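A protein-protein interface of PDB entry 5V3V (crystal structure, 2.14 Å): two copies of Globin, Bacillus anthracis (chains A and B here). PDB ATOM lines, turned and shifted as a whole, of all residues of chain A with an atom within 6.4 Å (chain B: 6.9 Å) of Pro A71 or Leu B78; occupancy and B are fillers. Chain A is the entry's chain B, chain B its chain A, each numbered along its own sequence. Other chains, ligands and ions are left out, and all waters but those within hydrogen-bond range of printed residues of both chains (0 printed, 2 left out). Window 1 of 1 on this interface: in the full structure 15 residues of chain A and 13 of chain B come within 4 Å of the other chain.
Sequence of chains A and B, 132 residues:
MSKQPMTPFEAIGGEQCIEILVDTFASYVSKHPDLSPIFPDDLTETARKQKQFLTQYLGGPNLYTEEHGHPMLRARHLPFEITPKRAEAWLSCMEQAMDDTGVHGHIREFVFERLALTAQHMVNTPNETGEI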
ATOM      1  N   PHE A  53       6.378 -27.802  19.310  1.00  0.00           N
ATOM      2  CA  PHE A  53       5.371 -27.015  20.017  1.00  0.00           C
ATOM      3  C   PHE A  53       3.971 -27.540  19.756  1.00  0.00           C
ATOM      4  O   PHE A  53       3.152 -27.610  20.682  1.00  0.00           O
ATOM      5  CB  PHE A  53       5.438 -25.539  19.632  1.00  0.00           C
ATOM      6  CG  PHE A  53       4.575 -24.667  20.500  1.00  0.00           C
ATOM      7  CD1 PHE A  53       5.072 -24.143  21.674  1.00  0.00           C
ATOM      8  CD2 PHE A  53       3.248 -24.405  20.161  1.00  0.00           C
ATOM      9  CE1 PHE A  53       4.279 -23.340  22.498  1.00  0.00           C
ATOM     10  CE2 PHE A  53       2.445 -23.599  20.973  1.00  0.00           C
ATOM     11  CZ  PHE A  53       2.964 -23.084  22.153  1.00  0.00           C
ATOM     12  N   GLN A  56       3.484 -30.803  21.801  1.00  0.00           N
ATOM     13  CA  GLN A  56       3.232 -30.584  23.219  1.00  0.00           C
ATOM     14  C   GLN A  56       1.908 -29.866  23.449  1.00  0.00           C
ATOM     15  O   GLN A  56       1.163 -30.207  24.378  1.00  0.00           O
ATOM     16  CB  GLN A  56       4.376 -29.795  23.841  1.00  0.00           C
ATOM     17  CG  GLN A  56       4.175 -29.513  25.327  1.00  0.00           C
ATOM     18  CD  GLN A  56       5.435 -28.996  25.969  1.00  0.00           C
ATOM     19  OE1 GLN A  56       6.413 -28.710  25.282  1.00  0.00           O
ATOM     20  NE2 GLN A  56       5.434 -28.895  27.288  1.00  0.00           N
ATOM     21  N   TYR A  57       1.593 -28.879  22.608  1.00  0.00           N
ATOM     22  CA  TYR A  57       0.353 -28.137  22.784  1.00  0.00           C
ATOM     23  C   TYR A  57      -0.866 -29.047  22.666  1.00  0.00           C
ATOM     24  O   TYR A  57      -1.860 -28.863  23.382  1.00  0.00           O
ATOM     25  CB  TYR A  57       0.283 -26.997  21.776  1.00  0.00           C
ATOM     26  CG  TYR A  57      -1.026 -26.241  21.805  1.00  0.00           C
ATOM     27  CD1 TYR A  57      -1.611 -25.849  23.012  1.00  0.00           C
ATOM     28  CD2 TYR A  57      -1.681 -25.913  20.621  1.00  0.00           C
ATOM     29  CE1 TYR A  57      -2.812 -25.159  23.034  1.00  0.00           C
ATOM     30  CE2 TYR A  57      -2.875 -25.221  20.634  1.00  0.00           C
ATOM     31  CZ  TYR A  57      -3.434 -24.846  21.845  1.00  0.00           C
ATOM     32  OH  TYR A  57      -4.624 -24.165  21.845  1.00  0.00           O
ATOM     33  N   TYR A  64       8.670 -29.432  23.355  1.00  0.00           N
ATOM     34  CA  TYR A  64       9.158 -28.058  23.272  1.00  0.00           C
ATOM     35  C   TYR A  64       9.756 -27.582  24.595  1.00  0.00           C
ATOM     36  O   TYR A  64      10.880 -27.067  24.615  1.00  0.00           O
ATOM     37  CB  TYR A  64       8.057 -27.107  22.821  1.00  0.00           C
ATOM     38  CG  TYR A  64       8.609 -25.721  22.594  1.00  0.00           C
ATOM     39  CD1 TYR A  64       8.756 -24.817  23.656  1.00  0.00           C
ATOM     40  CD2 TYR A  64       9.021 -25.320  21.326  1.00  0.00           C
ATOM     41  CE1 TYR A  64       9.297 -23.550  23.454  1.00  0.00           C
ATOM     42  CE2 TYR A  64       9.553 -24.039  21.104  1.00  0.00           C
ATOM     43  CZ  TYR A  64       9.685 -23.166  22.171  1.00  0.00           C
ATOM     44  OH  TYR A  64      10.205 -21.916  21.957  1.00  0.00           O
ATOM     45  N   THR A  65       9.012 -27.703  25.706  1.00  0.00           N
ATOM     46  CA  THR A  65       9.502 -27.128  26.959  1.00  0.00           C
ATOM     47  C   THR A  65      10.684 -27.912  27.512  1.00  0.00           C
ATOM     48  O   THR A  65      11.490 -27.360  28.278  1.00  0.00           O
ATOM     49  CB  THR A  65       8.388 -27.047  28.018  1.00  0.00           C
ATOM     50  OG1 THR A  65       7.809 -28.345  28.227  1.00  0.00           O
ATOM     51  CG2 THR A  65       7.309 -26.049  27.618  1.00  0.00           C
ATOM     52  N   HIS A  68      13.525 -26.102  25.288  1.00  0.00           N
ATOM     53  CA  HIS A  68      13.636 -24.655  25.202  1.00  0.00           C
ATOM     54  C   HIS A  68      13.124 -23.925  26.435  1.00  0.00           C
ATOM     55  O   HIS A  68      13.175 -22.691  26.468  1.00  0.00           O
ATOM     56  CB  HIS A  68      12.890 -24.153  23.961  1.00  0.00           C
ATOM     57  CG  HIS A  68      13.129 -24.982  22.738  1.00  0.00           C
ATOM     58  ND1 HIS A  68      14.268 -24.863  21.972  1.00  0.00           N
ATOM     59  CD2 HIS A  68      12.380 -25.947  22.155  1.00  0.00           C
ATOM     60  CE1 HIS A  68      14.205 -25.712  20.961  1.00  0.00           C
ATOM     61  NE2 HIS A  68      13.069 -26.384  21.051  1.00  0.00           N
ATOM     62  N   GLY A  69      12.630 -24.644  27.440  1.00  0.00           N
ATOM     63  CA  GLY A  69      12.102 -24.007  28.636  1.00  0.00           C
ATOM     64  C   GLY A  69      10.685 -23.488  28.452  1.00  0.00           C
ATOM     65  O   GLY A  69       9.914 -23.974  27.618  1.00  0.00           O
ATOM     66  N   HIS A  70      10.353 -22.470  29.237  1.00  0.00           N
ATOM     67  CA  HIS A  70       9.021 -21.882  29.188  1.00  0.00           C
ATOM     68  C   HIS A  70       8.697 -21.475  27.752  1.00  0.00           C
ATOM     69  O   HIS A  70       9.569 -20.959  27.056  1.00  0.00           O
ATOM     70  CB  HIS A  70       8.953 -20.666  30.114  1.00  0.00           C
ATOM     71  CG  HIS A  70       8.507 -20.986  31.501  1.00  0.00           C
ATOM     72  ND1 HIS A  70       7.829 -22.144  31.815  1.00  0.00           N
ATOM     73  CD2 HIS A  70       8.631 -20.297  32.658  1.00  0.00           C
ATOM     74  CE1 HIS A  70       7.562 -22.157  33.108  1.00  0.00           C
ATOM     75  NE2 HIS A  70       8.039 -21.048  33.643  1.00  0.00           N
ATOM     76  N   PRO A  71       7.477 -21.735  27.260  1.00  0.00           N
ATOM     77  CA  PRO A  71       7.192 -21.375  25.859  1.00  0.00           C
ATOM     78  C   PRO A  71       7.269 -19.883  25.624  1.00  0.00           C
ATOM     79  O   PRO A  71       7.890 -19.455  24.642  1.00  0.00           O
ATOM     80  CB  PRO A  71       5.776 -21.926  25.629  1.00  0.00           C
ATOM     81  CG  PRO A  71       5.186 -22.044  27.009  1.00  0.00           C
ATOM     82  CD  PRO A  71       6.341 -22.426  27.893  1.00  0.00           C
ATOM     83  N   MET A  72       6.669 -19.083  26.517  1.00  0.00           N
ATOM     84  CA  MET A  72       6.621 -17.612  26.410  1.00  0.00           C
ATOM     85  C   MET A  72       6.425 -17.163  24.957  1.00  0.00           C
ATOM     86  O   MET A  72       7.175 -16.344  24.414  1.00  0.00           O
ATOM     87  CB  MET A  72       7.875 -16.982  27.026  1.00  0.00           C
ATOM     88  CG  MET A  72       9.205 -17.371  26.360  1.00  0.00           C
ATOM     89  SD  MET A  72      10.607 -16.656  27.223  1.00  0.00           S
ATOM     90  CE  MET A  72      10.791 -17.841  28.548  1.00  0.00           C
ATOM     91  N   LEU A  73       5.380 -17.707  24.329  1.00  0.00           N
ATOM     92  CA  LEU A  73       5.326 -17.739  22.873  1.00  0.00           C
ATOM     93  C   LEU A  73       5.248 -16.343  22.275  1.00  0.00           C
ATOM     94  O   LEU A  73       5.929 -16.049  21.282  1.00  0.00           O
ATOM     95  CB  LEU A  73       4.136 -18.574  22.397  1.00  0.00           C
ATOM     96  CG  LEU A  73       4.209 -18.903  20.908  1.00  0.00           C
ATOM     97  CD1 LEU A  73       5.361 -19.870  20.634  1.00  0.00           C
ATOM     98  CD2 LEU A  73       2.870 -19.492  20.432  1.00  0.00           C
ATOM     99  N   ARG A  74       4.384 -15.482  22.829  1.00  0.00           N
ATOM    100  CA  ARG A  74       4.288 -14.133  22.286  1.00  0.00           C
ATOM    101  C   ARG A  74       5.628 -13.410  22.390  1.00  0.00           C
ATOM    102  O   ARG A  74       6.053 -12.736  21.444  1.00  0.00           O
ATOM    103  CB  ARG A  74       3.197 -13.336  22.987  1.00  0.00           C
ATOM    104  CG  ARG A  74       3.043 -11.960  22.364  1.00  0.00           C
ATOM    105  CD  ARG A  74       2.023 -11.097  23.055  1.00  0.00           C
ATOM    106  NE  ARG A  74       1.571 -10.044  22.149  1.00  0.00           N
ATOM    107  CZ  ARG A  74       1.988  -8.787  22.200  1.00  0.00           C
ATOM    108  NH1 ARG A  74       2.848  -8.412  23.135  1.00  0.00           N
ATOM    109  NH2 ARG A  74       1.530  -7.903  21.326  1.00  0.00           N
ATOM    110  N   ALA A  75       6.317 -13.560  23.523  1.00  0.00           N
ATOM    111  CA  ALA A  75       7.611 -12.905  23.694  1.00  0.00           C
ATOM    112  C   ALA A  75       8.605 -13.351  22.623  1.00  0.00           C
ATOM    113  O   ALA A  75       9.368 -12.533  22.093  1.00  0.00           O
ATOM    114  CB  ALA A  75       8.148 -13.188  25.094  1.00  0.00           C
ATOM    115  N   ARG A  76       8.594 -14.640  22.266  1.00  0.00           N
ATOM    116  CA  ARG A  76       9.502 -15.122  21.225  1.00  0.00           C
ATOM    117  C   ARG A  76       9.164 -14.545  19.862  1.00  0.00           C
ATOM    118  O   ARG A  76      10.026 -14.541  18.978  1.00  0.00           O
ATOM    119  CB  ARG A  76       9.473 -16.641  21.161  1.00  0.00           C
ATOM    120  CG  ARG A  76       9.934 -17.299  22.443  1.00  0.00           C
ATOM    121  CD  ARG A  76       9.989 -18.793  22.265  1.00  0.00           C
ATOM    122  NE  ARG A  76      10.266 -19.487  23.510  1.00  0.00           N
ATOM    123  CZ  ARG A  76      11.488 -19.751  23.978  1.00  0.00           C
ATOM    124  NH1 ARG A  76      12.579 -19.374  23.316  1.00  0.00           N
ATOM    125  NH2 ARG A  76      11.619 -20.403  25.122  1.00  0.00           N
ATOM    126  N   MET B  72      -5.182 -31.511  30.675  1.00  0.00           N
ATOM    127  CA  MET B  72      -3.804 -31.184  30.272  1.00  0.00           C
ATOM    128  C   MET B  72      -3.601 -29.674  30.224  1.00  0.00           C
ATOM    129  O   MET B  72      -3.130 -29.105  29.236  1.00  0.00           O
ATOM    130  CB  MET B  72      -3.450 -31.834  28.932  1.00  0.00           C
ATOM    131  CG  MET B  72      -3.493 -33.358  28.993  1.00  0.00           C
ATOM    132  SD  MET B  72      -2.550 -34.239  27.723  1.00  0.00           S
ATOM    133  CE  MET B  72      -0.887 -33.667  28.074  1.00  0.00           C
ATOM    134  N   LEU B  73      -4.003 -29.024  31.319  1.00  0.00           N
ATOM    135  CA  LEU B  73      -4.207 -27.582  31.292  1.00  0.00           C
ATOM    136  C   LEU B  73      -2.912 -26.832  31.054  1.00  0.00           C
ATOM    137  O   LEU B  73      -2.928 -25.773  30.427  1.00  0.00           O
ATOM    138  CB  LEU B  73      -4.859 -27.116  32.597  1.00  0.00           C
ATOM    139  CG  LEU B  73      -6.337 -27.397  32.830  1.00  0.00           C
ATOM    140  CD1 LEU B  73      -6.846 -26.536  33.979  1.00  0.00           C
ATOM    141  CD2 LEU B  73      -7.146 -27.130  31.577  1.00  0.00           C
ATOM    142  N   ARG B  74      -1.786 -27.348  31.540  1.00  0.00           N
ATOM    143  CA  ARG B  74      -0.525 -26.680  31.253  1.00  0.00           C
ATOM    144  C   ARG B  74      -0.216 -26.729  29.765  1.00  0.00           C
ATOM    145  O   ARG B  74       0.287 -25.751  29.202  1.00  0.00           O
ATOM    146  CB  ARG B  74       0.619 -27.292  32.061  1.00  0.00           C
ATOM    147  CG  ARG B  74       1.635 -26.243  32.471  1.00  0.00           C
ATOM    148  CD  ARG B  74       3.049 -26.772  32.644  1.00  0.00           C
ATOM    149  NE  ARG B  74       3.952 -26.221  31.628  1.00  0.00           N
ATOM    150  CZ  ARG B  74       4.363 -24.952  31.589  1.00  0.00           C
ATOM    151  NH1 ARG B  74       5.176 -24.545  30.617  1.00  0.00           N
ATOM    152  NH2 ARG B  74       3.961 -24.087  32.522  1.00  0.00           N
ATOM    153  N   ALA B  75      -0.531 -27.849  29.108  1.00  0.00           N
ATOM    154  CA  ALA B  75      -0.378 -27.924  27.656  1.00  0.00           C
ATOM    155  C   ALA B  75      -1.381 -27.020  26.938  1.00  0.00           C
ATOM    156  O   ALA B  75      -1.015 -26.307  26.004  1.00  0.00           O
ATOM    157  CB  ALA B  75      -0.519 -29.372  27.180  1.00  0.00           C
ATOM    158  N   ARG B  76      -2.641 -27.000  27.381  1.00  0.00           N
ATOM    159  CA  ARG B  76      -3.627 -26.150  26.718  1.00  0.00           C
ATOM    160  C   ARG B  76      -3.361 -24.665  26.900  1.00  0.00           C
ATOM    161  O   ARG B  76      -3.911 -23.859  26.143  1.00  0.00           O
ATOM    162  CB  ARG B  76      -5.027 -26.447  27.227  1.00  0.00           C
ATOM    163  CG  ARG B  76      -5.466 -27.870  27.018  1.00  0.00           C
ATOM    164  CD  ARG B  76      -6.961 -27.936  27.150  1.00  0.00           C
ATOM    165  NE  ARG B  76      -7.464 -29.301  27.186  1.00  0.00           N
ATOM    166  CZ  ARG B  76      -8.174 -29.863  26.218  1.00  0.00           C
ATOM    167  NH1 ARG B  76      -8.610 -31.109  26.360  1.00  0.00           N
ATOM    168  NH2 ARG B  76      -8.460 -29.172  25.119  1.00  0.00           N
ATOM    169  N   HIS B  77      -2.556 -24.275  27.887  1.00  0.00           N
ATOM    170  CA  HIS B  77      -2.244 -22.868  28.093  1.00  0.00           C
ATOM    171  C   HIS B  77      -0.890 -22.481  27.519  1.00  0.00           C
ATOM    172  O   HIS B  77      -0.471 -21.335  27.684  1.00  0.00           O
ATOM    173  CB  HIS B  77      -2.301 -22.525  29.589  1.00  0.00           C
ATOM    174  CG  HIS B  77      -3.690 -22.484  30.145  1.00  0.00           C
ATOM    175  ND1 HIS B  77      -4.405 -23.621  30.455  1.00  0.00           N
ATOM    176  CD2 HIS B  77      -4.502 -21.441  30.440  1.00  0.00           C
ATOM    177  CE1 HIS B  77      -5.593 -23.282  30.925  1.00  0.00           C
ATOM    178  NE2 HIS B  77      -5.680 -21.963  30.923  1.00  0.00           N
ATOM    179  N   LEU B  78      -0.204 -23.413  26.856  1.00  0.00           N
ATOM    180  CA  LEU B  78       1.119 -23.156  26.298  1.00  0.00           C
ATOM    181  C   LEU B  78       1.192 -21.917  25.417  1.00  0.00           C
ATOM    182  O   LEU B  78       2.183 -21.175  25.537  1.00  0.00           O
ATOM    183  CB  LEU B  78       1.588 -24.376  25.492  1.00  0.00           C
ATOM    184  CG  LEU B  78       2.509 -25.404  26.136  1.00  0.00           C
ATOM    185  CD1 LEU B  78       3.612 -25.750  25.154  1.00  0.00           C
ATOM    186  CD2 LEU B  78       3.084 -24.894  27.445  1.00  0.00           C
ATOM    187  N   PRO B  79       0.245 -21.648  24.506  1.00  0.00           N
ATOM    188  CA  PRO B  79       0.431 -20.498  23.609  1.00  0.00           C
ATOM    189  C   PRO B  79       0.093 -19.167  24.255  1.00  0.00           C
ATOM    190  O   PRO B  79       0.516 -18.122  23.740  1.00  0.00           O
ATOM    191  CB  PRO B  79      -0.504 -20.812  22.422  1.00  0.00           C
ATOM    192  CG  PRO B  79      -1.551 -21.693  22.982  1.00  0.00           C
ATOM    193  CD  PRO B  79      -0.937 -22.452  24.130  1.00  0.00           C
ATOM    194  N   PHE B  80      -0.609 -19.178  25.378  1.00  0.00           N
ATOM    195  CA  PHE B  80      -1.107 -17.959  25.992  1.00  0.00           C
ATOM    196  C   PHE B  80      -0.072 -17.354  26.924  1.00  0.00           C
ATOM    197  O   PHE B  80       0.628 -18.068  27.649  1.00  0.00           O
ATOM    198  CB  PHE B  80      -2.399 -18.257  26.749  1.00  0.00           C
ATOM    199  CG  PHE B  80      -3.404 -18.985  25.914  1.00  0.00           C
ATOM    200  CD1 PHE B  80      -3.667 -18.564  24.611  1.00  0.00           C
ATOM    201  CD2 PHE B  80      -4.056 -20.107  26.401  1.00  0.00           C
ATOM    202  CE1 PHE B  80      -4.583 -19.239  23.817  1.00  0.00           C
ATOM    203  CE2 PHE B  80      -4.967 -20.792  25.610  1.00  0.00           C
ATOM    204  CZ  PHE B  80      -5.235 -20.355  24.318  1.00  0.00           C
ATOM    205  N   GLU B  81       0.016 -16.029  26.905  1.00  0.00           N
ATOM    206  CA  GLU B  81       1.003 -15.323  27.713  1.00  0.00           C
ATOM    207  C   GLU B  81       0.534 -15.303  29.168  1.00  0.00           C
ATOM    208  O   GLU B  81      -0.165 -14.388  29.614  1.00  0.00           O
ATOM    209  CB  GLU B  81       1.228 -13.925  27.165  1.00  0.00           C
ATOM    210  CG  GLU B  81       2.224 -13.162  27.975  1.00  0.00           C
ATOM    211  CD  GLU B  81       2.698 -11.929  27.269  1.00  0.00           C
ATOM    212  OE1 GLU B  81       1.904 -10.966  27.155  1.00  0.00           O
ATOM    213  OE2 GLU B  81       3.864 -11.948  26.807  1.00  0.00           O
ATOM    214  N   ILE B  82       0.928 -16.321  29.931  1.00  0.00           N
ATOM    215  CA  ILE B  82       0.518 -16.431  31.325  1.00  0.00           C
ATOM    216  C   ILE B  82       1.723 -16.094  32.194  1.00  0.00           C
ATOM    217  O   ILE B  82       2.593 -16.935  32.448  1.00  0.00           O
ATOM    218  CB  ILE B  82      -0.060 -17.807  31.654  1.00  0.00           C
ATOM    219  CG1 ILE B  82      -1.266 -18.077  30.751  1.00  0.00           C
ATOM    220  CG2 ILE B  82      -0.477 -17.861  33.118  1.00  0.00           C
ATOM    221  CD1 ILE B  82      -1.994 -19.301  31.103  1.00  0.00           C
ATOM    222  N   MET B 122       0.185 -22.888  35.529  1.00  0.00           N
ATOM    223  CA  MET B 122      -0.104 -22.391  34.186  1.00  0.00           C
ATOM    224  C   MET B 122       0.926 -21.378  33.712  1.00  0.00           C
ATOM    225  O   MET B 122       1.124 -21.236  32.504  1.00  0.00           O
ATOM    226  CB  MET B 122      -1.511 -21.778  34.123  1.00  0.00           C
ATOM    227  CG  MET B 122      -2.667 -22.716  34.482  1.00  0.00           C
ATOM    228  SD  MET B 122      -2.783 -24.194  33.443  1.00  0.00           S
ATOM    229  CE  MET B 122      -1.866 -25.394  34.425  1.00  0.00           C
ATOM    230  N   VAL B 123       1.575 -20.669  34.639  1.00  0.00           N
ATOM    231  CA  VAL B 123       2.521 -19.600  34.323  1.00  0.00           C
ATOM    232  C   VAL B 123       3.593 -20.075  33.352  1.00  0.00           C
ATOM    233  O   VAL B 123       4.377 -20.976  33.668  1.00  0.00           O
ATOM    234  CB  VAL B 123       3.184 -19.042  35.596  1.00  0.00           C
ATOM    235  CG1 VAL B 123       4.321 -18.097  35.211  1.00  0.00           C
ATOM    236  CG2 VAL B 123       2.175 -18.330  36.465  1.00  0.00           C
ATOM    237  N   ASN B 124       3.672 -19.440  32.177  1.00  0.00           N
ATOM    238  CA  ASN B 124       4.566 -19.901  31.125  1.00  0.00           C
ATOM    239  C   ASN B 124       5.397 -18.762  30.538  1.00  0.00           C
ATOM    240  O   ASN B 124       5.913 -18.886  29.420  1.00  0.00           O
ATOM    241  CB  ASN B 124       3.766 -20.606  30.032  1.00  0.00           C
ATOM    242  CG  ASN B 124       2.652 -19.737  29.463  1.00  0.00           C
ATOM    243  OD1 ASN B 124       2.773 -18.515  29.380  1.00  0.00           O
ATOM    244  ND2 ASN B 124       1.564 -20.371  29.061  1.00  0.00           N
ATOM    245  N   THR B 125       5.526 -17.651  31.271  1.00  0.00           N
ATOM    246  CA  THR B 125       6.281 -16.482  30.859  1.00  0.00           C
ATOM    247  C   THR B 125       6.985 -15.933  32.093  1.00  0.00           C
ATOM    248  O   THR B 125       6.369 -15.847  33.167  1.00  0.00           O
ATOM    249  CB  THR B 125       5.369 -15.403  30.250  1.00  0.00           C
ATOM    250  OG1 THR B 125       4.543 -15.993  29.240  1.00  0.00           O
ATOM    251  CG2 THR B 125       6.188 -14.276  29.636  1.00  0.00           C
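The backbone NH (N) of Met A72 sits at hydrogen-bond distance from the backbone carbonyl oxygen (O) of Asn B124 (3.0 Å).
The guanidinium group (NH2) of Arg B74 sits at hydrogen-bond distance from the backbone carbonyl oxygen (O) of Val B123 (3.3 Å). The side-chain amide nitrogen (ND2) of Asn B124 sits at hydrogen-bond distance from the backbone carbonyl oxygen (O) of His B77, 2.6 Å away. O of Ile B82 sits at hydrogen-bond distance from N of Asn B124 (2.7 Å). The side-chain amide oxygen (OE1) of Gln A56 lies within hydrogen-bond range of the backbone NH (N) of Tyr A64 (3.1 Å). The side-chain hydroxyl (OG1) of Thr A65 is in hydrogen-bond range of the side-chain amide nitrogen (NE2) of Gln A56, at 2.6 Å. O of His A70 lies within hydrogen-bond range of NH2 of Arg A76, at 2.9 Å.
Among the printed residues, merely in contact across the chains: Tyr A57 with Ala B75, Gln A56 with Ala B75, His A70 with Val B123, Pro A71 with Leu B78, Tyr A57 with Pro B79, Tyr A57 with Arg B76, His A70 with Asn B124, Pro A71 with Asn B124, Pro A71 with Arg B74, Phe A53 with Leu B78, His A70 with Arg B74, Gln A56 with Leu B78, Met A72 with Thr B125, Phe A53 with Pro B79, Leu A73 with Pro B79 and Thr A65 with Arg B74.
Printed residues of chain B within 4 Å of Phe A53: Leu B78 (3.6 Å) and Pro B79 (3.9 Å). Printed residues of chain B within 4 Å of Thr A65: Arg B74. Pro A71 touches just these residues of chain B: Arg B74 (3.6 Å), Leu B78 (3.5 Å) and Asn B124 (3.6 Å). Leu B78 touches three residues of chain A. Of the printed residues of chain A, Pro B79 touches Phe A53, Tyr A57 and Leu A73. The nearest residue of chain B that does not touch Pro A71 is Pro B79 (5.6 Å).
Of the 15 printed residues of chain B, 8 touch a printed residue of chain A. Hydrophobic or aromatic side chains of chain B that line the printed part of chain A: Ala B75, Leu B78 and Pro B79. Of the 14 printed residues of chain A, 8 touch a printed residue of chain B. Hydrophobic or aromatic side chains of chain A that line the printed part of chain B: Phe A53, Tyr A57, His A70, Pro A71, Met A72 and Leu A73. Among the printed residues, no Asp or Glu carboxylate lies within 4 Å of a Lys or Arg side-chain nitrogen of the other chain.
Positions printed for both chains: 72, 73, 74, 75 and 76.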
